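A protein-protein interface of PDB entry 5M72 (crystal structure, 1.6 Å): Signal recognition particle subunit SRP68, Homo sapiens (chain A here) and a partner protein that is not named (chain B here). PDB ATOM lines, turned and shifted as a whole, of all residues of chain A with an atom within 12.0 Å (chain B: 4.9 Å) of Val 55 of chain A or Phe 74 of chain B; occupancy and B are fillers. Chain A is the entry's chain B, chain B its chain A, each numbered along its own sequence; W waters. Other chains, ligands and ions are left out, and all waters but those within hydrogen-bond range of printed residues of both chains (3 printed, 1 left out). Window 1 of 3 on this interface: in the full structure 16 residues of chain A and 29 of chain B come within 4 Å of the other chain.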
ATOM      1  N   PHE A  48       7.763 -40.414  -1.107  1.00  0.00           N
ATOM      2  CA  PHE A  48       6.526 -39.722  -0.745  1.00  0.00           C
ATOM      3  C   PHE A  48       6.397 -38.386  -1.467  1.00  0.00           C
ATOM      4  O   PHE A  48       7.347 -37.603  -1.527  1.00  0.00           O
ATOM      5  CB  PHE A  48       6.468 -39.473   0.765  1.00  0.00           C
ATOM      6  CG  PHE A  48       6.369 -40.726   1.585  1.00  0.00           C
ATOM      7  CD1 PHE A  48       7.507 -41.342   2.080  1.00  0.00           C
ATOM      8  CD2 PHE A  48       5.131 -41.276   1.875  1.00  0.00           C
ATOM      9  CE1 PHE A  48       7.411 -42.495   2.844  1.00  0.00           C
ATOM     10  CE2 PHE A  48       5.021 -42.424   2.632  1.00  0.00           C
ATOM     11  CZ  PHE A  48       6.163 -43.037   3.122  1.00  0.00           C
ATOM     12  N   ASP A  49       5.196 -38.102  -1.975  1.00  0.00           N
ATOM     13  CA  ASP A  49       4.898 -36.794  -2.561  1.00  0.00           C
ATOM     14  C   ASP A  49       4.560 -35.829  -1.428  1.00  0.00           C
ATOM     15  O   ASP A  49       3.395 -35.547  -1.130  1.00  0.00           O
ATOM     16  CB  ASP A  49       3.753 -36.907  -3.563  1.00  0.00           C
ATOM     17  CG  ASP A  49       3.336 -35.562  -4.159  1.00  0.00           C
ATOM     18  OD1 ASP A  49       4.015 -34.546  -3.915  1.00  0.00           O
ATOM     19  OD2 ASP A  49       2.319 -35.525  -4.893  1.00  0.00           O
ATOM     20  N   LEU A  50       5.607 -35.303  -0.786  1.00  0.00           N
ATOM     21  CA  LEU A  50       5.387 -34.357   0.303  1.00  0.00           C
ATOM     22  C   LEU A  50       4.936 -32.992  -0.202  1.00  0.00           C
ATOM     23  O   LEU A  50       4.315 -32.236   0.562  1.00  0.00           O
ATOM     24  CB  LEU A  50       6.655 -34.224   1.147  1.00  0.00           C
ATOM     25  CG  LEU A  50       7.050 -35.523   1.858  1.00  0.00           C
ATOM     26  CD1 LEU A  50       8.299 -35.319   2.692  1.00  0.00           C
ATOM     27  CD2 LEU A  50       5.915 -36.048   2.723  1.00  0.00           C
ATOM     28  N   ALA A  51       5.208 -32.670  -1.475  1.00  0.00           N
ATOM     29  CA  ALA A  51       4.733 -31.408  -2.039  1.00  0.00           C
ATOM     30  C   ALA A  51       3.218 -31.281  -1.928  1.00  0.00           C
ATOM     31  O   ALA A  51       2.698 -30.180  -1.727  1.00  0.00           O
ATOM     32  CB  ALA A  51       5.161 -31.281  -3.503  1.00  0.00           C
ATOM     33  N   LEU A  52       2.498 -32.395  -2.076  1.00  0.00           N
ATOM     34  CA  LEU A  52       1.042 -32.367  -1.962  1.00  0.00           C
ATOM     35  C   LEU A  52       0.578 -31.791  -0.627  1.00  0.00           C
ATOM     36  O   LEU A  52      -0.476 -31.136  -0.565  1.00  0.00           O
ATOM     37  CB  LEU A  52       0.481 -33.777  -2.159  1.00  0.00           C
ATOM     38  CG  LEU A  52      -1.043 -33.909  -2.113  1.00  0.00           C
ATOM     39  CD1 LEU A  52      -1.688 -32.971  -3.136  1.00  0.00           C
ATOM     40  CD2 LEU A  52      -1.424 -35.365  -2.386  1.00  0.00           C
ATOM     41  N   ASN A  53       1.343 -32.008   0.450  1.00  0.00           N
ATOM     42  CA  ASN A  53       0.935 -31.508   1.758  1.00  0.00           C
ATOM     43  C   ASN A  53       0.996 -29.991   1.837  1.00  0.00           C
ATOM     44  O   ASN A  53       0.342 -29.395   2.713  1.00  0.00           O
ATOM     45  CB  ASN A  53       1.806 -32.131   2.851  1.00  0.00           C
ATOM     46  CG  ASN A  53       1.608 -33.625   2.960  1.00  0.00           C
ATOM     47  OD1 ASN A  53       0.478 -34.121   2.884  1.00  0.00           O
ATOM     48  ND2 ASN A  53       2.703 -34.356   3.127  1.00  0.00           N
ATOM     49  N   HIS A  54       1.742 -29.361   0.933  1.00  0.00           N
ATOM     50  CA  HIS A  54       1.866 -27.912   0.878  1.00  0.00           C
ATOM     51  C   HIS A  54       0.750 -27.245   0.083  1.00  0.00           C
ATOM     52  O   HIS A  54       0.710 -26.014   0.028  1.00  0.00           O
ATOM     53  CB  HIS A  54       3.213 -27.517   0.254  1.00  0.00           C
ATOM     54  CG  HIS A  54       4.409 -27.961   1.035  1.00  0.00           C
ATOM     55  ND1 HIS A  54       4.907 -27.245   2.102  1.00  0.00           N
ATOM     56  CD2 HIS A  54       5.243 -29.017   0.870  1.00  0.00           C
ATOM     57  CE1 HIS A  54       5.978 -27.858   2.580  1.00  0.00           C
ATOM     58  NE2 HIS A  54       6.198 -28.939   1.855  1.00  0.00           N
ATOM     59  N   VAL A  55      -0.136 -28.014  -0.554  1.00  0.00           N
ATOM     60  CA  VAL A  55      -1.169 -27.444  -1.417  1.00  0.00           C
ATOM     61  C   VAL A  55      -2.295 -26.960  -0.508  1.00  0.00           C
ATOM     62  O   VAL A  55      -3.077 -27.757   0.008  1.00  0.00           O
ATOM     63  CB  VAL A  55      -1.675 -28.449  -2.455  1.00  0.00           C
ATOM     64  CG1 VAL A  55      -2.803 -27.826  -3.296  1.00  0.00           C
ATOM     65  CG2 VAL A  55      -0.507 -28.932  -3.370  1.00  0.00           C
ATOM     66  N   ALA A  56      -2.367 -25.651  -0.293  1.00  0.00           N
ATOM     67  CA  ALA A  56      -3.278 -25.107   0.702  1.00  0.00           C
ATOM     68  C   ALA A  56      -3.682 -23.695   0.315  1.00  0.00           C
ATOM     69  O   ALA A  56      -2.949 -22.997  -0.388  1.00  0.00           O
ATOM     70  CB  ALA A  56      -2.630 -25.099   2.095  1.00  0.00           C
ATOM     71  N   PHE A  57      -4.850 -23.272   0.803  1.00  0.00           N
ATOM     72  CA  PHE A  57      -5.290 -21.904   0.578  1.00  0.00           C
ATOM     73  C   PHE A  57      -4.264 -20.916   1.130  1.00  0.00           C
ATOM     74  O   PHE A  57      -3.628 -21.173   2.159  1.00  0.00           O
ATOM     75  CB  PHE A  57      -6.629 -21.632   1.268  1.00  0.00           C
ATOM     76  CG  PHE A  57      -7.806 -22.341   0.663  1.00  0.00           C
ATOM     77  CD1 PHE A  57      -7.714 -22.999  -0.558  1.00  0.00           C
ATOM     78  CD2 PHE A  57      -9.038 -22.319   1.323  1.00  0.00           C
ATOM     79  CE1 PHE A  57      -8.815 -23.640  -1.088  1.00  0.00           C
ATOM     80  CE2 PHE A  57     -10.129 -22.956   0.799  1.00  0.00           C
ATOM     81  CZ  PHE A  57     -10.029 -23.616  -0.413  1.00  0.00           C
ATOM     82  N   PRO A  58      -4.116 -19.760   0.493  1.00  0.00           N
ATOM     83  CA  PRO A  58      -3.381 -18.654   1.113  1.00  0.00           C
ATOM     84  C   PRO A  58      -4.149 -18.107   2.304  1.00  0.00           C
ATOM     85  O   PRO A  58      -5.324 -18.454   2.499  1.00  0.00           O
ATOM     86  CB  PRO A  58      -3.291 -17.618  -0.018  1.00  0.00           C
ATOM     87  CG  PRO A  58      -4.509 -17.887  -0.852  1.00  0.00           C
ATOM     88  CD  PRO A  58      -4.688 -19.387  -0.816  1.00  0.00           C
ATOM     89  N   PRO A  59      -3.521 -17.270   3.130  1.00  0.00           N
ATOM     90  CA  PRO A  59      -4.240 -16.664   4.262  1.00  0.00           C
ATOM     91  C   PRO A  59      -5.426 -15.843   3.777  1.00  0.00           C
ATOM     92  O   PRO A  59      -5.309 -15.056   2.836  1.00  0.00           O
ATOM     93  CB  PRO A  59      -3.174 -15.782   4.923  1.00  0.00           C
ATOM     94  CG  PRO A  59      -1.870 -16.417   4.533  1.00  0.00           C
ATOM     95  CD  PRO A  59      -2.079 -16.962   3.153  1.00  0.00           C
ATOM     96  N   LEU A  60      -6.575 -16.017   4.444  1.00  0.00           N
ATOM     97  CA  LEU A  60      -7.830 -15.432   3.987  1.00  0.00           C
ATOM     98  C   LEU A  60      -8.362 -14.335   4.895  1.00  0.00           C
ATOM     99  O   LEU A  60      -9.445 -13.808   4.619  1.00  0.00           O
ATOM    100  CB  LEU A  60      -8.903 -16.520   3.838  1.00  0.00           C
ATOM    101  CG  LEU A  60      -8.623 -17.650   2.845  1.00  0.00           C
ATOM    102  CD1 LEU A  60      -9.820 -18.586   2.756  1.00  0.00           C
ATOM    103  CD2 LEU A  60      -8.260 -17.095   1.471  1.00  0.00           C
ATOM    104  N   VAL B  45      -6.263 -24.541  -5.781  1.00  0.00           N
ATOM    105  CA  VAL B  45      -6.031 -25.467  -4.670  1.00  0.00           C
ATOM    106  C   VAL B  45      -7.150 -26.499  -4.580  1.00  0.00           C
ATOM    107  O   VAL B  45      -6.896 -27.695  -4.391  1.00  0.00           O
ATOM    108  CB  VAL B  45      -5.875 -24.697  -3.345  1.00  0.00           C
ATOM    109  CG1 VAL B  45      -5.884 -25.659  -2.160  1.00  0.00           C
ATOM    110  CG2 VAL B  45      -4.594 -23.881  -3.366  1.00  0.00           C
ATOM    111  N   ILE B  48      -6.751 -29.077  -7.351  1.00  0.00           N
ATOM    112  CA  ILE B  48      -5.641 -29.993  -7.070  1.00  0.00           C
ATOM    113  C   ILE B  48      -6.021 -30.972  -5.971  1.00  0.00           C
ATOM    114  O   ILE B  48      -5.730 -32.177  -6.059  1.00  0.00           O
ATOM    115  CB  ILE B  48      -4.374 -29.206  -6.698  1.00  0.00           C
ATOM    116  CG1 ILE B  48      -3.858 -28.404  -7.902  1.00  0.00           C
ATOM    117  CG2 ILE B  48      -3.264 -30.156  -6.174  1.00  0.00           C
ATOM    118  CD1 ILE B  48      -2.748 -27.402  -7.561  1.00  0.00           C
ATOM    119  N   GLN B  49      -6.684 -30.473  -4.922  1.00  0.00           N
ATOM    120  CA  GLN B  49      -7.075 -31.322  -3.801  1.00  0.00           C
ATOM    121  C   GLN B  49      -8.058 -32.408  -4.214  1.00  0.00           C
ATOM    122  O   GLN B  49      -8.130 -33.450  -3.553  1.00  0.00           O
ATOM    123  CB  GLN B  49      -7.675 -30.466  -2.674  1.00  0.00           C
ATOM    124  CG  GLN B  49      -6.635 -29.679  -1.869  1.00  0.00           C
ATOM    125  CD  GLN B  49      -5.795 -30.572  -0.984  1.00  0.00           C
ATOM    126  OE1 GLN B  49      -6.175 -31.708  -0.699  1.00  0.00           O
ATOM    127  NE2 GLN B  49      -4.635 -30.074  -0.556  1.00  0.00           N
ATOM    128  N   LEU B  72       1.215 -18.403  -8.809  1.00  0.00           N
ATOM    129  CA  LEU B  72       1.071 -19.759  -8.326  1.00  0.00           C
ATOM    130  C   LEU B  72       2.076 -20.649  -9.040  1.00  0.00           C
ATOM    131  O   LEU B  72       1.714 -21.666  -9.627  1.00  0.00           O
ATOM    132  CB  LEU B  72      -0.363 -20.244  -8.535  1.00  0.00           C
ATOM    133  CG  LEU B  72      -1.397 -19.102  -8.519  1.00  0.00           C
ATOM    134  CD1 LEU B  72      -2.779 -19.575  -8.907  1.00  0.00           C
ATOM    135  CD2 LEU B  72      -1.440 -18.400  -7.166  1.00  0.00           C
ATOM    136  N   SER B  73       3.351 -20.238  -9.037  1.00  0.00           N
ATOM    137  CA  SER B  73       4.380 -21.054  -9.681  1.00  0.00           C
ATOM    138  C   SER B  73       4.451 -22.440  -9.057  1.00  0.00           C
ATOM    139  O   SER B  73       4.608 -23.438  -9.770  1.00  0.00           O
ATOM    140  CB  SER B  73       5.748 -20.378  -9.605  1.00  0.00           C
ATOM    141  OG  SER B  73       5.895 -19.412 -10.633  1.00  0.00           O
ATOM    142  N   PHE B  74       4.325 -22.521  -7.725  1.00  0.00           N
ATOM    143  CA  PHE B  74       4.282 -23.823  -7.064  1.00  0.00           C
ATOM    144  C   PHE B  74       3.134 -24.667  -7.599  1.00  0.00           C
ATOM    145  O   PHE B  74       3.331 -25.819  -7.996  1.00  0.00           O
ATOM    146  CB  PHE B  74       4.157 -23.658  -5.548  1.00  0.00           C
ATOM    147  CG  PHE B  74       3.843 -24.946  -4.831  1.00  0.00           C
ATOM    148  CD1 PHE B  74       4.788 -25.965  -4.778  1.00  0.00           C
ATOM    149  CD2 PHE B  74       2.599 -25.154  -4.248  1.00  0.00           C
ATOM    150  CE1 PHE B  74       4.506 -27.163  -4.135  1.00  0.00           C
ATOM    151  CE2 PHE B  74       2.310 -26.352  -3.596  1.00  0.00           C
ATOM    152  CZ  PHE B  74       3.272 -27.361  -3.546  1.00  0.00           C
ATOM    153  N   GLU B  75       1.923 -24.106  -7.621  1.00  0.00           N
ATOM    154  CA  GLU B  75       0.766 -24.877  -8.059  1.00  0.00           C
ATOM    155  C   GLU B  75       0.874 -25.256  -9.531  1.00  0.00           C
ATOM    156  O   GLU B  75       0.532 -26.382  -9.913  1.00  0.00           O
ATOM    157  CB  GLU B  75      -0.521 -24.088  -7.794  1.00  0.00           C
ATOM    158  CG  GLU B  75      -0.913 -23.989  -6.312  1.00  0.00           C
ATOM    159  CD  GLU B  75      -0.178 -22.880  -5.551  1.00  0.00           C
ATOM    160  OE1 GLU B  75       0.647 -22.165  -6.164  1.00  0.00           O
ATOM    161  OE2 GLU B  75      -0.436 -22.719  -4.333  1.00  0.00           O
ATOM    162  N   LYS B  76       1.352 -24.335 -10.373  1.00  0.00           N
ATOM    163  CA  LYS B  76       1.499 -24.637 -11.794  1.00  0.00           C
ATOM    164  C   LYS B  76       2.505 -25.761 -12.008  1.00  0.00           C
ATOM    165  O   LYS B  76       2.238 -26.721 -12.745  1.00  0.00           O
ATOM    166  CB  LYS B  76       1.922 -23.380 -12.557  1.00  0.00           C
ATOM    167  CG  LYS B  76       2.232 -23.590 -14.036  1.00  0.00           C
ATOM    168  CD  LYS B  76       2.528 -22.255 -14.721  1.00  0.00           C
ATOM    169  CE  LYS B  76       2.729 -22.408 -16.224  1.00  0.00           C
ATOM    170  NZ  LYS B  76       4.044 -23.027 -16.548  1.00  0.00           N
ATOM    171  N   ALA B  77       3.667 -25.661 -11.362  1.00  0.00           N
ATOM    172  CA  ALA B  77       4.671 -26.717 -11.478  1.00  0.00           C
ATOM    173  C   ALA B  77       4.165 -28.028 -10.887  1.00  0.00           C
ATOM    174  O   ALA B  77       4.477 -29.113 -11.408  1.00  0.00           O
ATOM    175  CB  ALA B  77       5.969 -26.289 -10.788  1.00  0.00           C
ATOM    176  N   TYR B  78       3.390 -27.953  -9.799  1.00  0.00           N
ATOM    177  CA  TYR B  78       2.861 -29.171  -9.195  1.00  0.00           C
ATOM    178  C   TYR B  78       1.936 -29.897 -10.170  1.00  0.00           C
ATOM    179  O   TYR B  78       2.037 -31.119 -10.351  1.00  0.00           O
ATOM    180  CB  TYR B  78       2.134 -28.858  -7.871  1.00  0.00           C
ATOM    181  CG  TYR B  78       1.742 -30.141  -7.193  1.00  0.00           C
ATOM    182  CD1 TYR B  78       2.695 -30.934  -6.582  1.00  0.00           C
ATOM    183  CD2 TYR B  78       0.429 -30.609  -7.236  1.00  0.00           C
ATOM    184  CE1 TYR B  78       2.358 -32.141  -6.001  1.00  0.00           C
ATOM    185  CE2 TYR B  78       0.084 -31.809  -6.663  1.00  0.00           C
ATOM    186  CZ  TYR B  78       1.058 -32.579  -6.046  1.00  0.00           C
ATOM    187  OH  TYR B  78       0.736 -33.786  -5.482  1.00  0.00           O
ATOM    188  N   LYS B 102       7.696 -24.474  -0.219  1.00  0.00           N
ATOM    189  CA  LYS B 102       6.906 -25.378  -1.058  1.00  0.00           C
ATOM    190  C   LYS B 102       7.609 -25.657  -2.376  1.00  0.00           C
ATOM    191  O   LYS B 102       7.627 -26.794  -2.867  1.00  0.00           O
ATOM    192  CB  LYS B 102       5.530 -24.774  -1.356  1.00  0.00           C
ATOM    193  CG  LYS B 102       4.706 -24.301  -0.179  1.00  0.00           C
ATOM    194  CD  LYS B 102       3.358 -23.811  -0.695  1.00  0.00           C
ATOM    195  CE  LYS B 102       2.456 -23.342   0.433  1.00  0.00           C
ATOM    196  NZ  LYS B 102       1.125 -22.886  -0.062  1.00  0.00           N
ATOM    197  N   LEU B 103       8.163 -24.610  -2.990  1.00  0.00           N
ATOM    198  CA  LEU B 103       8.873 -24.795  -4.255  1.00  0.00           C
ATOM    199  C   LEU B 103      10.093 -25.683  -4.069  1.00  0.00           C
ATOM    200  O   LEU B 103      10.412 -26.504  -4.939  1.00  0.00           O
ATOM    201  CB  LEU B 103       9.274 -23.443  -4.842  1.00  0.00           C
ATOM    202  CG  LEU B 103       8.182 -22.703  -5.617  1.00  0.00           C
ATOM    203  CD1 LEU B 103       8.591 -21.260  -5.854  1.00  0.00           C
ATOM    204  CD2 LEU B 103       7.888 -23.411  -6.939  1.00  0.00           C
ATOM    205  N   LEU B 106       9.005 -29.413  -3.834  1.00  0.00           N
ATOM    206  CA  LEU B 106       8.718 -29.947  -5.157  1.00  0.00           C
ATOM    207  C   LEU B 106       9.992 -30.081  -5.986  1.00  0.00           C
ATOM    208  O   LEU B 106      10.154 -31.051  -6.739  1.00  0.00           O
ATOM    209  CB  LEU B 106       7.692 -29.051  -5.859  1.00  0.00           C
ATOM    210  CG  LEU B 106       7.258 -29.510  -7.253  1.00  0.00           C
ATOM    211  CD1 LEU B 106       6.648 -30.913  -7.204  1.00  0.00           C
ATOM    212  CD2 LEU B 106       6.277 -28.506  -7.865  1.00  0.00           C
HETATM  213  O   HOH W   1      -2.835 -31.819   0.883  1.00  0.00           O
HETATM  214  O   HOH W   2      -4.696 -27.851   2.115  1.00  0.00           O
HETATM  215  O   HOH W   3      -0.815 -21.216  -0.001  1.00  0.00           O
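The side-chain amide nitrogen (NE2) of Gln 49 of chain B lies within hydrogen-bond range of the backbone carbonyl oxygen (O) of Val 55 of chain A.
OD2 of Asp 49 of chain A sits at hydrogen-bond distance from OH of Tyr 78 of chain B, 2.4 Å away.
The backbone carbonyl oxygen of His 54 of chain A sits at hydrogen-bond distance from the side-chain amino group of Lys 102 of chain B (3.2 Å).
N of Ala 51 of chain A sits close to OD1 of Asp 49 of chain A (3.3 Å).
The side-chain carboxylate (OD1) of Asp 49 of chain A sits at hydrogen-bond distance from the backbone NH (N) of Leu 52 of chain A (3.2 Å).
Ala 51 of chain A touches Phe 74 of chain B.
Ala 51 of chain A touches Tyr 78 of chain B.
CB of Leu 52 of chain A touches OH of Tyr 78 of chain B, at 3.3 Å.
CB of His 54 of chain A touches CZ of Phe 74 of chain B, at 3.8 Å.
CG1 of Val 55 of chain A touches CG1 of Val 45 of chain B, 3.9 Å away.
CG1 of Val 55 of chain A touches CG2 of Ile 48 of chain B (3.7 Å).
Phe 74 of chain B touches Val 55 of chain A (CE2 to CG2, 3.8 Å).
Ala 56 of chain A touches Val 45 of chain B.
Val 45 of chain B touches Phe 57 of chain A.
Val 55 of chain A touches four residues of chain B.
Of chain A, only Ala 51 (3.4 Å), His 54 (3.8 Å) and Val 55 (3.8 Å) come within 4 Å of Phe 74 of chain B.
Of chain A, only Val 55 (3.9 Å), Ala 56 (3.5 Å) and Phe 57 (3.6 Å) come within 4 Å of Val 45 of chain B.
Of chain A, only Val 55 comes within 4 Å of Ile 48 of chain B.
Of chain A, only Val 55 comes within 4 Å of Gln 49 of chain B.
No residue of chain A comes within 4 Å of Glu 75 of chain B.
No residue of chain A comes within 4 Å of Leu 103 of chain B.
Of the printed residues of chain B, Asp 49 of chain A touches Tyr 78.
Of the printed residues of chain B, Leu 52 of chain A touches Tyr 78.
Of the printed residues of chain B, Phe 57 of chain A touches Val 45 (3.6 Å).
Printed residues of chain B within 4 Å of Ala 56 of chain A: Val 45 (3.5 Å).
Of the printed residues of chain A, Lys 102 of chain B touches His 54.
Leu 60 of chain A touches none of the printed residues of chain B.
The nearest residue of chain B that does not touch Val 55 of chain A is Tyr 78 of chain B (4.3 Å).
Printed residues of chain B that touch a printed residue of chain A: Val 45, Ile 48, Gln 49, Phe 74, Tyr 78 and Lys 102.
Hydrophobic or aromatic side chains of chain B that line the printed part of chain A: Val 45, Ile 48, Phe 74 and Tyr 78.
Along chain B the printed residues that touch a printed residue of chain A span positions 45 to 102.
Water W3 lies within hydrogen-bond range of NZ of Lys 102 of chain B (2.6 Å) and O of Ala 56 of chain A (2.8 Å).
Water W2 bridges O of Val 55 of chain A (2.7 Å) and NE2 of Gln 49 of chain B (3.5 Å).
Water W1 lies within hydrogen-bond range of the backbone carbonyl oxygen (O) of Leu 52 of chain A (2.9 Å) and the side-chain amide nitrogen (NE2) of Gln 49 of chain B (2.9 Å).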
